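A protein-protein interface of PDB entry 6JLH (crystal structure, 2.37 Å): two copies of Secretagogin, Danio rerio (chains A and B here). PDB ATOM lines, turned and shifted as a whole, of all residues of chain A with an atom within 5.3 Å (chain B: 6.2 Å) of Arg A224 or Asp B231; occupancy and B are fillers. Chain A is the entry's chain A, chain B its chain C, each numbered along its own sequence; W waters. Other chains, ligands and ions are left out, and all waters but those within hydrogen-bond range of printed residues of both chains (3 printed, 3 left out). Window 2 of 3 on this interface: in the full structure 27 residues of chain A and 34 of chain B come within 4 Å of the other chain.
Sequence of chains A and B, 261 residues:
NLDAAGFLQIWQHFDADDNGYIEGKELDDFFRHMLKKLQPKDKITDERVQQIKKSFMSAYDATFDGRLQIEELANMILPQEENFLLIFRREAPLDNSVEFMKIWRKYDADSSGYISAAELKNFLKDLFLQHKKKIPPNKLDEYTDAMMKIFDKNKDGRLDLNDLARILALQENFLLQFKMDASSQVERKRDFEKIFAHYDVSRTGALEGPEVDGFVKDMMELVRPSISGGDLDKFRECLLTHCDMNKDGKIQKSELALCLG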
ATOM      1  N   MET A 220      10.559  17.211  16.305  1.00  0.00           N
ATOM      2  CA  MET A 220       9.122  17.337  16.126  1.00  0.00           C
ATOM      3  C   MET A 220       8.687  18.819  16.147  1.00  0.00           C
ATOM      4  O   MET A 220       7.770  19.198  15.396  1.00  0.00           O
ATOM      5  CB  MET A 220       8.374  16.508  17.172  1.00  0.00           C
ATOM      6  CG  MET A 220       8.651  15.008  17.109  1.00  0.00           C
ATOM      7  SD  MET A 220       8.366  14.272  15.336  1.00  0.00           S
ATOM      8  CE  MET A 220       6.500  14.667  14.851  1.00  0.00           C
ATOM      9  N   GLU A 221       9.347  19.661  16.966  1.00  0.00           N
ATOM     10  CA  GLU A 221       8.920  21.043  17.144  1.00  0.00           C
ATOM     11  C   GLU A 221       9.361  21.925  15.957  1.00  0.00           C
ATOM     12  O   GLU A 221       8.994  23.083  15.943  1.00  0.00           O
ATOM     13  CB  GLU A 221       9.376  21.596  18.495  1.00  0.00           C
ATOM     14  CG  GLU A 221       8.607  20.986  19.642  1.00  0.00           C
ATOM     15  CD  GLU A 221       9.016  21.434  21.041  1.00  0.00           C
ATOM     16  OE1 GLU A 221       8.385  20.978  22.012  1.00  0.00           O
ATOM     17  OE2 GLU A 221       9.930  22.268  21.167  1.00  0.00           O
ATOM     18  N   LEU A 222      10.125  21.388  15.003  1.00  0.00           N
ATOM     19  CA  LEU A 222      10.401  22.059  13.706  1.00  0.00           C
ATOM     20  C   LEU A 222       9.104  22.188  12.912  1.00  0.00           C
ATOM     21  O   LEU A 222       9.059  23.109  12.081  1.00  0.00           O
ATOM     22  CB  LEU A 222      11.401  21.266  12.851  1.00  0.00           C
ATOM     23  CG  LEU A 222      12.826  21.170  13.389  1.00  0.00           C
ATOM     24  CD1 LEU A 222      13.647  20.265  12.501  1.00  0.00           C
ATOM     25  CD2 LEU A 222      13.483  22.540  13.516  1.00  0.00           C
ATOM     26  N   VAL A 223       8.135  21.284  13.087  1.00  0.00           N
ATOM     27  CA  VAL A 223       6.953  21.230  12.171  1.00  0.00           C
ATOM     28  C   VAL A 223       5.634  21.395  12.931  1.00  0.00           C
ATOM     29  O   VAL A 223       4.599  21.516  12.299  1.00  0.00           O
ATOM     30  CB  VAL A 223       6.955  19.932  11.360  1.00  0.00           C
ATOM     31  CG1 VAL A 223       8.270  19.783  10.635  1.00  0.00           C
ATOM     32  CG2 VAL A 223       6.650  18.717  12.212  1.00  0.00           C
ATOM     33  N   ARG A 224       5.671  21.315  14.255  1.00  0.00           N
ATOM     34  CA  ARG A 224       4.406  21.432  15.022  1.00  0.00           C
ATOM     35  C   ARG A 224       4.650  22.238  16.294  1.00  0.00           C
ATOM     36  O   ARG A 224       5.819  22.419  16.666  1.00  0.00           O
ATOM     37  CB  ARG A 224       3.801  20.057  15.321  1.00  0.00           C
ATOM     38  CG  ARG A 224       4.811  19.004  15.747  1.00  0.00           C
ATOM     39  CD  ARG A 224       4.253  18.062  16.796  1.00  0.00           C
ATOM     40  NE  ARG A 224       2.801  17.977  16.785  1.00  0.00           N
ATOM     41  CZ  ARG A 224       2.091  17.208  15.969  1.00  0.00           C
ATOM     42  NH1 ARG A 224       2.693  16.446  15.071  1.00  0.00           N
ATOM     43  NH2 ARG A 224       0.775  17.210  16.048  1.00  0.00           N
ATOM     44  N   PRO A 225       3.595  22.775  16.939  1.00  0.00           N
ATOM     45  CA  PRO A 225       3.785  23.524  18.182  1.00  0.00           C
ATOM     46  C   PRO A 225       4.277  22.630  19.340  1.00  0.00           C
ATOM     47  O   PRO A 225       4.424  21.431  19.186  1.00  0.00           O
ATOM     48  CB  PRO A 225       2.402  24.139  18.403  1.00  0.00           C
ATOM     49  CG  PRO A 225       1.439  23.206  17.699  1.00  0.00           C
ATOM     50  CD  PRO A 225       2.197  22.626  16.535  1.00  0.00           C
ATOM     51  N   SER A 226       4.638  23.232  20.460  1.00  0.00           N
ATOM     52  CA  SER A 226       5.222  22.517  21.621  1.00  0.00           C
ATOM     53  C   SER A 226       4.466  21.204  21.883  1.00  0.00           C
ATOM     54  O   SER A 226       3.243  21.272  22.091  1.00  0.00           O
ATOM     55  CB  SER A 226       5.229  23.421  22.818  1.00  0.00           C
ATOM     56  OG  SER A 226       5.998  24.587  22.552  1.00  0.00           O
ATOM     57  N   ILE A 227       5.161  20.069  21.890  1.00  0.00           N
ATOM     58  CA  ILE A 227       4.576  18.708  22.118  1.00  0.00           C
ATOM     59  C   ILE A 227       4.382  18.386  23.615  1.00  0.00           C
ATOM     60  O   ILE A 227       5.043  18.951  24.500  1.00  0.00           O
ATOM     61  CB  ILE A 227       5.440  17.603  21.470  1.00  0.00           C
ATOM     62  CG1 ILE A 227       6.786  17.415  22.173  1.00  0.00           C
ATOM     63  CG2 ILE A 227       5.610  17.847  19.980  1.00  0.00           C
ATOM     64  CD1 ILE A 227       7.455  16.115  21.826  1.00  0.00           C
ATOM     65  N   PHE A 235       6.509   9.648  19.862  1.00  0.00           N
ATOM     66  CA  PHE A 235       7.420   9.955  18.729  1.00  0.00           C
ATOM     67  C   PHE A 235       8.800   9.336  18.989  1.00  0.00           C
ATOM     68  O   PHE A 235       9.492   8.944  18.022  1.00  0.00           O
ATOM     69  CB  PHE A 235       7.503  11.465  18.480  1.00  0.00           C
ATOM     70  CG  PHE A 235       6.220  12.071  17.971  1.00  0.00           C
ATOM     71  CD1 PHE A 235       5.591  11.541  16.865  1.00  0.00           C
ATOM     72  CD2 PHE A 235       5.642  13.174  18.586  1.00  0.00           C
ATOM     73  CE1 PHE A 235       4.415  12.087  16.373  1.00  0.00           C
ATOM     74  CE2 PHE A 235       4.471  13.733  18.093  1.00  0.00           C
ATOM     75  CZ  PHE A 235       3.861  13.193  16.981  1.00  0.00           C
ATOM     76  N   TYR B 114      -2.497  24.615   7.643  1.00  0.00           N
ATOM     77  CA  TYR B 114      -1.441  25.641   7.814  1.00  0.00           C
ATOM     78  C   TYR B 114      -1.793  26.875   6.976  1.00  0.00           C
ATOM     79  O   TYR B 114      -2.396  26.721   5.893  1.00  0.00           O
ATOM     80  CB  TYR B 114      -0.113  25.134   7.272  1.00  0.00           C
ATOM     81  CG  TYR B 114       0.636  24.077   8.045  1.00  0.00           C
ATOM     82  CD1 TYR B 114       1.240  24.350   9.274  1.00  0.00           C
ATOM     83  CD2 TYR B 114       0.863  22.826   7.486  1.00  0.00           C
ATOM     84  CE1 TYR B 114       1.982  23.389   9.959  1.00  0.00           C
ATOM     85  CE2 TYR B 114       1.611  21.859   8.152  1.00  0.00           C
ATOM     86  CZ  TYR B 114       2.167  22.136   9.391  1.00  0.00           C
ATOM     87  OH  TYR B 114       2.901  21.169  10.023  1.00  0.00           O
ATOM     88  N   ASN B 154       8.775  28.193  14.344  1.00  0.00           N
ATOM     89  CA  ASN B 154       9.666  27.056  14.012  1.00  0.00           C
ATOM     90  C   ASN B 154      10.206  27.176  12.566  1.00  0.00           C
ATOM     91  O   ASN B 154      10.879  26.228  12.083  1.00  0.00           O
ATOM     92  CB  ASN B 154       8.946  25.744  14.339  1.00  0.00           C
ATOM     93  CG  ASN B 154       7.644  25.600  13.586  1.00  0.00           C
ATOM     94  OD1 ASN B 154       7.335  26.435  12.738  1.00  0.00           O
ATOM     95  ND2 ASN B 154       6.856  24.587  13.926  1.00  0.00           N
ATOM     96  N   ASP B 156       9.166  27.179   9.382  1.00  0.00           N
ATOM     97  CA  ASP B 156       8.803  26.299   8.233  1.00  0.00           C
ATOM     98  C   ASP B 156       8.075  27.100   7.148  1.00  0.00           C
ATOM     99  O   ASP B 156       7.580  26.457   6.220  1.00  0.00           O
ATOM    100  CB  ASP B 156       7.960  25.094   8.664  1.00  0.00           C
ATOM    101  CG  ASP B 156       6.663  25.425   9.390  1.00  0.00           C
ATOM    102  OD1 ASP B 156       6.314  26.600   9.476  1.00  0.00           O
ATOM    103  OD2 ASP B 156       6.030  24.487   9.912  1.00  0.00           O
ATOM    104  N   ASP B 160       0.744  28.030  11.975  1.00  0.00           N
ATOM    105  CA  ASP B 160      -0.110  26.969  12.531  1.00  0.00           C
ATOM    106  C   ASP B 160      -1.296  27.628  13.250  1.00  0.00           C
ATOM    107  O   ASP B 160      -1.388  28.883  13.361  1.00  0.00           O
ATOM    108  CB  ASP B 160       0.698  26.051  13.448  1.00  0.00           C
ATOM    109  CG  ASP B 160       0.291  24.593  13.350  1.00  0.00           C
ATOM    110  OD1 ASP B 160      -0.901  24.307  13.002  1.00  0.00           O
ATOM    111  OD2 ASP B 160       1.179  23.756  13.577  1.00  0.00           O
ATOM    112  N   VAL B 216     -13.717  20.998  19.532  1.00  0.00           N
ATOM    113  CA  VAL B 216     -12.634  19.977  19.530  1.00  0.00           C
ATOM    114  C   VAL B 216     -11.338  20.634  20.020  1.00  0.00           C
ATOM    115  O   VAL B 216     -10.644  20.039  20.867  1.00  0.00           O
ATOM    116  CB  VAL B 216     -12.469  19.325  18.139  1.00  0.00           C
ATOM    117  CG1 VAL B 216     -11.177  18.538  18.004  1.00  0.00           C
ATOM    118  CG2 VAL B 216     -13.631  18.417  17.816  1.00  0.00           C
ATOM    119  N   MET B 220      -9.792  19.358  23.502  1.00  0.00           N
ATOM    120  CA  MET B 220      -8.437  18.758  23.483  1.00  0.00           C
ATOM    121  C   MET B 220      -7.486  19.588  24.369  1.00  0.00           C
ATOM    122  O   MET B 220      -6.649  18.998  25.070  1.00  0.00           O
ATOM    123  CB  MET B 220      -7.936  18.607  22.037  1.00  0.00           C
ATOM    124  CG  MET B 220      -8.737  17.668  21.156  1.00  0.00           C
ATOM    125  SD  MET B 220      -9.124  15.906  22.006  1.00  0.00           S
ATOM    126  CE  MET B 220      -7.393  15.138  22.405  1.00  0.00           C
ATOM    127  N   ARG B 224      -4.049  18.817  26.956  1.00  0.00           N
ATOM    128  CA  ARG B 224      -2.752  18.885  26.252  1.00  0.00           C
ATOM    129  C   ARG B 224      -2.456  20.334  25.905  1.00  0.00           C
ATOM    130  O   ARG B 224      -3.316  21.204  26.032  1.00  0.00           O
ATOM    131  CB  ARG B 224      -2.755  17.913  25.069  1.00  0.00           C
ATOM    132  CG  ARG B 224      -3.937  18.038  24.135  1.00  0.00           C
ATOM    133  CD  ARG B 224      -3.629  17.690  22.699  1.00  0.00           C
ATOM    134  NE  ARG B 224      -2.725  16.568  22.581  1.00  0.00           N
ATOM    135  CZ  ARG B 224      -1.414  16.660  22.307  1.00  0.00           C
ATOM    136  NH1 ARG B 224      -0.704  15.548  22.249  1.00  0.00           N
ATOM    137  NH2 ARG B 224      -0.804  17.832  22.133  1.00  0.00           N
ATOM    138  N   SER B 226      -1.541  23.676  23.445  1.00  0.00           N
ATOM    139  CA  SER B 226      -2.140  24.191  22.196  1.00  0.00           C
ATOM    140  C   SER B 226      -1.904  23.200  21.042  1.00  0.00           C
ATOM    141  O   SER B 226      -0.727  22.907  20.746  1.00  0.00           O
ATOM    142  CB  SER B 226      -1.541  25.559  21.881  1.00  0.00           C
ATOM    143  OG  SER B 226      -1.700  26.479  22.969  1.00  0.00           O
ATOM    144  N   ILE B 227      -2.965  22.764  20.355  1.00  0.00           N
ATOM    145  CA  ILE B 227      -2.926  21.792  19.219  1.00  0.00           C
ATOM    146  C   ILE B 227      -2.689  22.490  17.864  1.00  0.00           C
ATOM    147  O   ILE B 227      -2.950  23.727  17.739  1.00  0.00           O
ATOM    148  CB  ILE B 227      -4.210  20.937  19.136  1.00  0.00           C
ATOM    149  CG1 ILE B 227      -5.438  21.731  18.677  1.00  0.00           C
ATOM    150  CG2 ILE B 227      -4.479  20.213  20.451  1.00  0.00           C
ATOM    151  CD1 ILE B 227      -6.598  20.848  18.228  1.00  0.00           C
ATOM    152  N   SER B 228      -2.287  21.680  16.871  1.00  0.00           N
ATOM    153  CA  SER B 228      -1.964  22.086  15.497  1.00  0.00           C
ATOM    154  C   SER B 228      -3.199  22.026  14.610  1.00  0.00           C
ATOM    155  O   SER B 228      -4.231  21.446  15.036  1.00  0.00           O
ATOM    156  CB  SER B 228      -0.908  21.187  14.931  1.00  0.00           C
ATOM    157  OG  SER B 228      -1.460  19.928  14.574  1.00  0.00           O
ATOM    158  N   GLY B 229      -3.062  22.548  13.384  1.00  0.00           N
ATOM    159  CA  GLY B 229      -4.107  22.434  12.359  1.00  0.00           C
ATOM    160  C   GLY B 229      -4.386  20.983  12.017  1.00  0.00           C
ATOM    161  O   GLY B 229      -5.538  20.638  11.893  1.00  0.00           O
ATOM    162  N   GLY B 230      -3.346  20.178  11.814  1.00  0.00           N
ATOM    163  CA  GLY B 230      -3.444  18.732  11.511  1.00  0.00           C
ATOM    164  C   GLY B 230      -4.101  17.980  12.656  1.00  0.00           C
ATOM    165  O   GLY B 230      -4.975  17.159  12.394  1.00  0.00           O
ATOM    166  N   ASP B 231      -3.698  18.284  13.890  1.00  0.00           N
ATOM    167  CA  ASP B 231      -4.280  17.717  15.131  1.00  0.00           C
ATOM    168  C   ASP B 231      -5.786  17.979  15.168  1.00  0.00           C
ATOM    169  O   ASP B 231      -6.536  17.077  15.579  1.00  0.00           O
ATOM    170  CB  ASP B 231      -3.688  18.370  16.379  1.00  0.00           C
ATOM    171  CG  ASP B 231      -2.241  18.040  16.645  1.00  0.00           C
ATOM    172  OD1 ASP B 231      -1.784  17.015  16.082  1.00  0.00           O
ATOM    173  OD2 ASP B 231      -1.605  18.801  17.443  1.00  0.00           O
ATOM    174  N   LEU B 232      -6.190  19.199  14.811  1.00  0.00           N
ATOM    175  CA  LEU B 232      -7.611  19.586  14.783  1.00  0.00           C
ATOM    176  C   LEU B 232      -8.379  18.652  13.857  1.00  0.00           C
ATOM    177  O   LEU B 232      -9.408  18.140  14.294  1.00  0.00           O
ATOM    178  CB  LEU B 232      -7.768  21.036  14.331  1.00  0.00           C
ATOM    179  CG  LEU B 232      -9.222  21.474  14.201  1.00  0.00           C
ATOM    180  CD1 LEU B 232      -9.861  21.604  15.546  1.00  0.00           C
ATOM    181  CD2 LEU B 232      -9.322  22.766  13.469  1.00  0.00           C
ATOM    182  N   ASP B 233      -7.924  18.476  12.620  1.00  0.00           N
ATOM    183  CA  ASP B 233      -8.612  17.605  11.618  1.00  0.00           C
ATOM    184  C   ASP B 233      -8.623  16.141  12.123  1.00  0.00           C
ATOM    185  O   ASP B 233      -9.665  15.447  11.946  1.00  0.00           O
ATOM    186  CB  ASP B 233      -8.022  17.794  10.223  1.00  0.00           C
ATOM    187  CG  ASP B 233      -8.366  19.126   9.550  1.00  0.00           C
ATOM    188  OD1 ASP B 233      -9.497  19.592   9.665  1.00  0.00           O
ATOM    189  OD2 ASP B 233      -7.510  19.671   8.864  1.00  0.00           O
ATOM    190  N   LYS B 234      -7.569  15.689  12.794  1.00  0.00           N
ATOM    191  CA  LYS B 234      -7.478  14.297  13.308  1.00  0.00           C
ATOM    192  C   LYS B 234      -8.544  14.079  14.383  1.00  0.00           C
ATOM    193  O   LYS B 234      -9.352  13.148  14.247  1.00  0.00           O
ATOM    194  CB  LYS B 234      -6.076  14.027  13.868  1.00  0.00           C
ATOM    195  CG  LYS B 234      -5.864  12.617  14.419  1.00  0.00           C
ATOM    196  CD  LYS B 234      -4.437  12.370  14.864  1.00  0.00           C
ATOM    197  CE  LYS B 234      -4.174  12.992  16.220  1.00  0.00           C
ATOM    198  NZ  LYS B 234      -2.728  13.121  16.537  1.00  0.00           N
ATOM    199  N   PHE B 235      -8.576  14.953  15.389  1.00  0.00           N
ATOM    200  CA  PHE B 235      -9.454  14.805  16.568  1.00  0.00           C
ATOM    201  C   PHE B 235     -10.903  15.093  16.166  1.00  0.00           C
ATOM    202  O   PHE B 235     -11.830  14.488  16.762  1.00  0.00           O
ATOM    203  CB  PHE B 235      -8.936  15.683  17.705  1.00  0.00           C
ATOM    204  CG  PHE B 235      -7.639  15.204  18.318  1.00  0.00           C
ATOM    205  CD1 PHE B 235      -7.494  13.898  18.756  1.00  0.00           C
ATOM    206  CD2 PHE B 235      -6.569  16.066  18.471  1.00  0.00           C
ATOM    207  CE1 PHE B 235      -6.314  13.461  19.332  1.00  0.00           C
ATOM    208  CE2 PHE B 235      -5.381  15.636  19.044  1.00  0.00           C
ATOM    209  CZ  PHE B 235      -5.263  14.335  19.484  1.00  0.00           C
ATOM    210  N   ARG B 236     -11.106  15.967  15.179  1.00  0.00           N
ATOM    211  CA  ARG B 236     -12.452  16.246  14.635  1.00  0.00           C
ATOM    212  C   ARG B 236     -13.026  14.947  14.054  1.00  0.00           C
ATOM    213  O   ARG B 236     -14.123  14.538  14.428  1.00  0.00           O
ATOM    214  CB  ARG B 236     -12.354  17.354  13.590  1.00  0.00           C
ATOM    215  CG  ARG B 236     -13.676  17.726  12.955  1.00  0.00           C
ATOM    216  CD  ARG B 236     -13.491  18.722  11.824  1.00  0.00           C
ATOM    217  NE  ARG B 236     -14.691  19.544  11.713  1.00  0.00           N
ATOM    218  CZ  ARG B 236     -15.800  19.197  11.077  1.00  0.00           C
ATOM    219  NH1 ARG B 236     -15.869  18.048  10.436  1.00  0.00           N
ATOM    220  NH2 ARG B 236     -16.843  19.999  11.086  1.00  0.00           N
HETATM  221  O   HOH W   1       0.642  18.867  13.291  1.00  0.00           O
HETATM  222  O   HOH W   2       1.635  23.522  22.023  1.00  0.00           O
HETATM  223  O   HOH W   3       1.616  21.239  12.540  1.00  0.00           O
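Printed residues of chain B within 4 Å of Glu A221: Asn B154 (3.1 Å).
Of the printed residues of chain A, Ser B228 touches Arg A224 and Pro A225.
Leu B232 touches none of the printed residues of chain A.
Lys B234 touches none of the printed residues of chain A.
The nearest printed residue of chain B that does not touch Glu A221 is Asp B156 (6.9 Å).
Water W1 lies within hydrogen-bond range of OG of Ser B228 and NH2 of Arg A224.
Water W2 lies within hydrogen-bond range of O of Ser B226 (2.8 Å) and O of Ser A226 (2.8 Å).
Water W3 lies within hydrogen-bond range of the side-chain carboxylate of Asp B160, the side-chain hydroxyl of Tyr B114 and the backbone carbonyl oxygen of Val A223.
The side-chain carboxylate (OE1) of Glu A221 is in hydrogen-bond range of the backbone NH (N) of Ile A227 (3.4 Å).
N of Gly B229 is in hydrogen-bond range of OD1 of Asp B160, at 2.8 Å.
The backbone NH (N) of Gly B230 lies within hydrogen-bond range of the side-chain hydroxyl (OG) of Ser B228 (3.4 Å).
The backbone NH of Asp B231 lies within hydrogen-bond range of the side-chain hydroxyl of Ser B228, 2.9 Å away.
5 positions are printed for both chains.
Of the 11 pairs that touch across the chains among the printed residues, none has its exchanged pair printed and touching as well.
The backbone carbonyl oxygen of Glu A221 lies close to the side-chain amide nitrogen of Asn B154, at 3.3 Å.
The backbone carbonyl oxygen (O) of Leu A222 is in hydrogen-bond range of the side-chain amide nitrogen (ND2) of Asn B154, at 3.2 Å.
The backbone carbonyl oxygen (O) of Val A223 sits at hydrogen-bond distance from the side-chain hydroxyl (OH) of Tyr B114 (2.9 Å).
The side-chain amide nitrogen (ND2) of Asn B154 sits close to the backbone NH (N) of Arg A224.
The side-chain carboxylate (OD1) of Asp B231 lies within salt-bridge range of the guanidinium group (NH2) of Arg A224 (2.6 Å).
Along chain A the printed residues that touch a printed residue of chain B span positions 221 to 225.
Among the printed residues, 11 pairs touch across the chains.
Among the printed residues, Asp or Glu carboxylates within 4 Å of a Lys or Arg side-chain nitrogen of the other chain: Arg A224 with Asp B231 (2.6 Å).
Leu A222 touches Asp B156.
Val A223 touches Asn B154 (C to ND2, 3.6 Å).
Arg A224 touches Ser B228 (NH2 to OG, 3.8 Å).
Pro A225 touches Asp B160.
Pro A225 touches Ser B226 (CG to O, 3.8 Å).
Pro A225 touches Ser B228 (CD to CB, 3.8 Å).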
